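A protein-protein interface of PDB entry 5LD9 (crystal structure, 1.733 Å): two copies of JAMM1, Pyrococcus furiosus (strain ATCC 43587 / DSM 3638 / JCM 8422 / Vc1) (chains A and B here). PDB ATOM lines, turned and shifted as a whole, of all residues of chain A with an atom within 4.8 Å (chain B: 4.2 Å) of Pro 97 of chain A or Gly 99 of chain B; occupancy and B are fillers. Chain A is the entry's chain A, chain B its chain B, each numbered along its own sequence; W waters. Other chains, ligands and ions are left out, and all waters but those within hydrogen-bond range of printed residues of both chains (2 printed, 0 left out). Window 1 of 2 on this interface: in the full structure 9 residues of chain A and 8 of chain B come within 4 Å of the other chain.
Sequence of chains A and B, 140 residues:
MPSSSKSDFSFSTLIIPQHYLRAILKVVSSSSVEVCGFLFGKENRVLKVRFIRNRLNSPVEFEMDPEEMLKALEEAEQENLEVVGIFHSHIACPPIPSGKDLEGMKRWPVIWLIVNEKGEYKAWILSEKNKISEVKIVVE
Ser 98 of chain B touches Ser 98 of chain A.
Gly 99 of chain B touches Ser 98 of chain A (N to C, 3.4 Å).
N of Gly 99 of chain A touches C of Ser 98 of chain B, 3.7 Å away.
CA of Gly 99 of chain A touches CD1 of Leu 102 of chain B, 3.5 Å away.
Gly 99 of chain B touches Leu 102 of chain A.
C of Gly 99 of chain B touches CD1 of Ile 132 of chain A, at 3.6 Å.
Ile 132 of chain A touches Lys 100 of chain B.
Of the 11 printed residues of chain A, 5 touch a printed residue of chain B.
Of the 6 printed residues of chain B, 5 touch a printed residue of chain A.
Hydrophobic or aromatic side chains of chain B within 4 Å of the printed part of chain A: Leu 102.
Along chain B the printed residues that touch a printed residue of chain A span positions 98 to 103.
Among the printed residues, 10 pairs touch across the chains.
Ser 98 of chain A touches its own counterpart, Ser 98 of chain B.
Ser 98 of chain A touches Gly 99 of chain B, and with the chains exchanged Gly 99 of chain A touches Ser 98 of chain B.
Gly 99 of chain A touches its own counterpart, Gly 99 of chain B.
Gly 99 of chain A touches Leu 102 of chain B, and with the chains exchanged Leu 102 of chain A touches Gly 99 of chain B.
Of the 10 pairs that touch across the chains among the printed residues, 6 have their exchanged pair printed and touching as well.
OG of Ser 98 of chain B is in hydrogen-bond range of N of Asp 101 of chain B, 2.9 Å away.
The backbone NH (N) of Lys 100 of chain B sits close to the side-chain hydroxyl (OG) of Ser 98 of chain B.
The side-chain hydroxyl of Ser 98 of chain A sits at hydrogen-bond distance from the backbone NH of Asp 101 of chain A.
Water W1 bridges the backbone carbonyl oxygen of Ile 132 of chain A (2.6 Å) and the side-chain carboxylate of Glu 103 of chain B (2.8 Å).
Water W2 lies within hydrogen-bond range of the backbone carbonyl oxygen of Pro 97 of chain A (2.6 Å), the backbone NH of Lys 100 of chain B (3.0 Å) and the backbone NH of Gly 99 of chain B (3.3 Å).
Of the printed residues of chain B, Pro 97 of chain A touches Gly 99 (3.0 Å).
Gly 99 of chain B touches just these residues of chain A: Pro 97, Ser 98, Gly 99, Leu 102 and Ile 132.
Of the printed residues of chain B, Leu 102 of chain A touches Gly 99.
Of the printed residues of chain A, Leu 102 of chain B touches Gly 99 (3.5 Å).
Printed residues of chain B within 4 Å of Gly 99 of chain A: Ser 98, Gly 99 and Leu 102.
The nearest printed residue of chain A that does not touch Gly 99 of chain B is Ile 96 of chain A (6.3 Å).
The nearest printed residue of chain B that does not touch Leu 102 of chain A is Leu 102 of chain B (4.1 Å).
N of Ile 132 of chain A sits at hydrogen-bond distance from OE2 of Glu 103 of chain B.
N of Gly 99 of chain B sits close to N of Gly 99 of chain A.
The backbone carbonyl oxygen (O) of Pro 97 of chain A sits at hydrogen-bond distance from the backbone NH (N) of Gly 99 of chain B, 3.0 Å away.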
ATOM      1  N   PRO A  95       7.754   6.636 -12.677  1.00  0.00           N
ATOM      2  CA  PRO A  95       7.374   6.008 -13.953  1.00  0.00           C
ATOM      3  C   PRO A  95       6.603   6.967 -14.856  1.00  0.00           C
ATOM      4  O   PRO A  95       5.443   6.733 -15.224  1.00  0.00           O
ATOM      5  CB  PRO A  95       6.528   4.814 -13.485  1.00  0.00           C
ATOM      6  CG  PRO A  95       5.873   5.293 -12.238  1.00  0.00           C
ATOM      7  CD  PRO A  95       6.865   6.231 -11.572  1.00  0.00           C
ATOM      8  N   ILE A  96       7.264   8.067 -15.218  1.00  0.00           N
ATOM      9  CA  ILE A  96       6.665   9.174 -15.964  1.00  0.00           C
ATOM     10  C   ILE A  96       7.512   9.395 -17.214  1.00  0.00           C
ATOM     11  O   ILE A  96       8.737   9.263 -17.148  1.00  0.00           O
ATOM     12  CB  ILE A  96       6.583  10.435 -15.085  1.00  0.00           C
ATOM     13  CG1 ILE A  96       5.783  10.126 -13.807  1.00  0.00           C
ATOM     14  CG2 ILE A  96       5.933  11.574 -15.823  1.00  0.00           C
ATOM     15  CD1 ILE A  96       5.796  11.224 -12.767  1.00  0.00           C
ATOM     16  N   PRO A  97       6.931   9.725 -18.370  1.00  0.00           N
ATOM     17  CA  PRO A  97       7.739   9.783 -19.596  1.00  0.00           C
ATOM     18  C   PRO A  97       8.872  10.803 -19.515  1.00  0.00           C
ATOM     19  O   PRO A  97       8.670  11.960 -19.143  1.00  0.00           O
ATOM     20  CB  PRO A  97       6.722  10.180 -20.673  1.00  0.00           C
ATOM     21  CG  PRO A  97       5.419   9.706 -20.145  1.00  0.00           C
ATOM     22  CD  PRO A  97       5.503   9.942 -18.654  1.00  0.00           C
ATOM     23  N   SER A  98      10.065  10.354 -19.892  1.00  0.00           N
ATOM     24  CA  SER A  98      11.198  11.230 -20.125  1.00  0.00           C
ATOM     25  C   SER A  98      10.996  11.979 -21.437  1.00  0.00           C
ATOM     26  O   SER A  98      10.052  11.721 -22.193  1.00  0.00           O
ATOM     27  CB  SER A  98      12.492  10.423 -20.184  1.00  0.00           C
ATOM     28  OG  SER A  98      12.526   9.640 -21.371  1.00  0.00           O
ATOM     29  N   GLY A  99      11.907  12.912 -21.720  1.00  0.00           N
ATOM     30  CA  GLY A  99      11.855  13.597 -22.998  1.00  0.00           C
ATOM     31  C   GLY A  99      12.080  12.654 -24.165  1.00  0.00           C
ATOM     32  O   GLY A  99      11.412  12.756 -25.201  1.00  0.00           O
ATOM     33  N   ASP A 101      11.358   9.488 -24.096  1.00  0.00           N
ATOM     34  CA  ASP A 101      10.148   8.677 -24.177  1.00  0.00           C
ATOM     35  C   ASP A 101       9.088   9.371 -25.019  1.00  0.00           C
ATOM     36  O   ASP A 101       8.405   8.723 -25.824  1.00  0.00           O
ATOM     37  CB  ASP A 101       9.593   8.386 -22.791  1.00  0.00           C
ATOM     38  CG  ASP A 101      10.467   7.453 -21.979  1.00  0.00           C
ATOM     39  OD1 ASP A 101      11.281   6.681 -22.534  1.00  0.00           O
ATOM     40  OD2 ASP A 101      10.333   7.520 -20.761  1.00  0.00           O
ATOM     41  N   LEU A 102       8.932  10.688 -24.845  1.00  0.00           N
ATOM     42  CA  LEU A 102       7.934  11.426 -25.617  1.00  0.00           C
ATOM     43  C   LEU A 102       8.218  11.327 -27.107  1.00  0.00           C
ATOM     44  O   LEU A 102       7.297  11.143 -27.910  1.00  0.00           O
ATOM     45  CB  LEU A 102       7.893  12.894 -25.190  1.00  0.00           C
ATOM     46  CG  LEU A 102       6.951  13.788 -26.006  1.00  0.00           C
ATOM     47  CD1 LEU A 102       5.519  13.276 -25.913  1.00  0.00           C
ATOM     48  CD2 LEU A 102       7.038  15.237 -25.553  1.00  0.00           C
ATOM     49  N   MET A 105       6.990   8.042 -28.102  1.00  0.00           N
ATOM     50  CA  MET A 105       5.535   7.924 -28.082  1.00  0.00           C
ATOM     51  C   MET A 105       4.912   8.522 -29.334  1.00  0.00           C
ATOM     52  O   MET A 105       3.844   8.072 -29.769  1.00  0.00           O
ATOM     53  CB  MET A 105       4.974   8.603 -26.832  1.00  0.00           C
ATOM     54  CG  MET A 105       5.258   7.865 -25.530  1.00  0.00           C
ATOM     55  SD  MET A 105       4.725   8.811 -24.091  1.00  0.00           S
ATOM     56  CE  MET A 105       2.953   8.607 -24.150  1.00  0.00           C
ATOM     57  N   ILE A 114       5.144   2.232 -18.006  1.00  0.00           N
ATOM     58  CA  ILE A 114       6.425   2.509 -17.373  1.00  0.00           C
ATOM     59  C   ILE A 114       6.368   2.001 -15.943  1.00  0.00           C
ATOM     60  O   ILE A 114       5.383   2.240 -15.233  1.00  0.00           O
ATOM     61  CB  ILE A 114       6.782   4.002 -17.412  1.00  0.00           C
ATOM     62  CG1 ILE A 114       6.573   4.548 -18.832  1.00  0.00           C
ATOM     63  CG2 ILE A 114       8.209   4.186 -16.924  1.00  0.00           C
ATOM     64  CD1 ILE A 114       6.966   6.039 -18.988  1.00  0.00           C
ATOM     65  N   TRP A 124       0.683   5.552 -20.148  1.00  0.00           N
ATOM     66  CA  TRP A 124       0.621   6.858 -20.789  1.00  0.00           C
ATOM     67  C   TRP A 124       0.302   6.699 -22.264  1.00  0.00           C
ATOM     68  O   TRP A 124       0.714   5.732 -22.909  1.00  0.00           O
ATOM     69  CB  TRP A 124       1.953   7.609 -20.672  1.00  0.00           C
ATOM     70  CG  TRP A 124       2.429   7.669 -19.274  1.00  0.00           C
ATOM     71  CD1 TRP A 124       3.274   6.797 -18.654  1.00  0.00           C
ATOM     72  CD2 TRP A 124       2.044   8.629 -18.297  1.00  0.00           C
ATOM     73  NE1 TRP A 124       3.454   7.168 -17.341  1.00  0.00           N
ATOM     74  CE2 TRP A 124       2.704   8.287 -17.094  1.00  0.00           C
ATOM     75  CE3 TRP A 124       1.199   9.744 -18.313  1.00  0.00           C
ATOM     76  CZ2 TRP A 124       2.563   9.037 -15.936  1.00  0.00           C
ATOM     77  CZ3 TRP A 124       1.058  10.480 -17.162  1.00  0.00           C
ATOM     78  CH2 TRP A 124       1.732  10.122 -15.983  1.00  0.00           C
ATOM     79  N   ILE A 132       0.770  14.308 -23.558  1.00  0.00           N
ATOM     80  CA  ILE A 132       0.891  13.192 -22.631  1.00  0.00           C
ATOM     81  C   ILE A 132      -0.335  13.140 -21.740  1.00  0.00           C
ATOM     82  O   ILE A 132      -0.703  14.129 -21.093  1.00  0.00           O
ATOM     83  CB  ILE A 132       2.171  13.327 -21.794  1.00  0.00           C
ATOM     84  CG1 ILE A 132       3.411  13.232 -22.684  1.00  0.00           C
ATOM     85  CG2 ILE A 132       2.223  12.239 -20.716  1.00  0.00           C
ATOM     86  CD1 ILE A 132       4.689  13.704 -21.981  1.00  0.00           C
ATOM     87  N   SER B  98      11.810  16.571 -18.751  1.00  0.00           N
ATOM     88  CA  SER B  98      10.855  15.481 -18.861  1.00  0.00           C
ATOM     89  C   SER B  98      10.038  15.635 -20.141  1.00  0.00           C
ATOM     90  O   SER B  98      10.129  16.636 -20.849  1.00  0.00           O
ATOM     91  CB  SER B  98       9.911  15.479 -17.662  1.00  0.00           C
ATOM     92  OG  SER B  98       9.110  16.654 -17.672  1.00  0.00           O
ATOM     93  N   GLY B  99       9.204  14.637 -20.431  1.00  0.00           N
ATOM     94  CA  GLY B  99       8.290  14.793 -21.550  1.00  0.00           C
ATOM     95  C   GLY B  99       7.358  15.979 -21.366  1.00  0.00           C
ATOM     96  O   GLY B  99       7.141  16.762 -22.294  1.00  0.00           O
ATOM     97  N   LYS B 100       6.792  16.127 -20.166  1.00  0.00           N
ATOM     98  CA  LYS B 100       5.931  17.274 -19.889  1.00  0.00           C
ATOM     99  C   LYS B 100       6.710  18.584 -19.946  1.00  0.00           C
ATOM    100  O   LYS B 100       6.166  19.611 -20.377  1.00  0.00           O
ATOM    101  CB  LYS B 100       5.247  17.103 -18.526  1.00  0.00           C
ATOM    102  CG  LYS B 100       4.311  15.886 -18.429  1.00  0.00           C
ATOM    103  CD  LYS B 100       2.883  16.286 -18.063  1.00  0.00           C
ATOM    104  CE  LYS B 100       1.974  15.075 -17.855  1.00  0.00           C
ATOM    105  NZ  LYS B 100       2.315  14.296 -16.626  1.00  0.00           N
ATOM    106  N   ASP B 101       7.990  18.566 -19.560  1.00  0.00           N
ATOM    107  CA  ASP B 101       8.824  19.757 -19.706  1.00  0.00           C
ATOM    108  C   ASP B 101       8.957  20.166 -21.172  1.00  0.00           C
ATOM    109  O   ASP B 101       8.884  21.356 -21.498  1.00  0.00           O
ATOM    110  CB  ASP B 101      10.212  19.520 -19.106  1.00  0.00           C
ATOM    111  CG  ASP B 101      10.218  19.506 -17.572  1.00  0.00           C
ATOM    112  OD1 ASP B 101       9.255  19.987 -16.935  1.00  0.00           O
ATOM    113  OD2 ASP B 101      11.211  19.011 -16.997  1.00  0.00           O
ATOM    114  N   LEU B 102       9.169  19.195 -22.071  1.00  0.00           N
ATOM    115  CA  LEU B 102       9.267  19.504 -23.499  1.00  0.00           C
ATOM    116  C   LEU B 102       7.979  20.121 -24.025  1.00  0.00           C
ATOM    117  O   LEU B 102       8.012  20.992 -24.904  1.00  0.00           O
ATOM    118  CB  LEU B 102       9.601  18.239 -24.298  1.00  0.00           C
ATOM    119  CG  LEU B 102      10.968  17.599 -24.039  1.00  0.00           C
ATOM    120  CD1 LEU B 102      11.173  16.388 -24.929  1.00  0.00           C
ATOM    121  CD2 LEU B 102      12.093  18.603 -24.252  1.00  0.00           C
ATOM    122  N   GLU B 103       6.827  19.656 -23.531  1.00  0.00           N
ATOM    123  CA  GLU B 103       5.570  20.284 -23.916  1.00  0.00           C
ATOM    124  C   GLU B 103       5.535  21.738 -23.464  1.00  0.00           C
ATOM    125  O   GLU B 103       5.079  22.619 -24.204  1.00  0.00           O
ATOM    126  CB  GLU B 103       4.392  19.500 -23.333  1.00  0.00           C
ATOM    127  CG  GLU B 103       4.317  18.062 -23.823  1.00  0.00           C
ATOM    128  CD  GLU B 103       3.117  17.309 -23.269  1.00  0.00           C
ATOM    129  OE1 GLU B 103       2.559  17.747 -22.241  1.00  0.00           O
ATOM    130  OE2 GLU B 103       2.728  16.291 -23.861  1.00  0.00           O
HETATM  131  O   HOH W   1       0.419  16.468 -20.952  1.00  0.00           O
HETATM  132  O   HOH W   2       6.763  13.637 -18.473  1.00  0.00           O
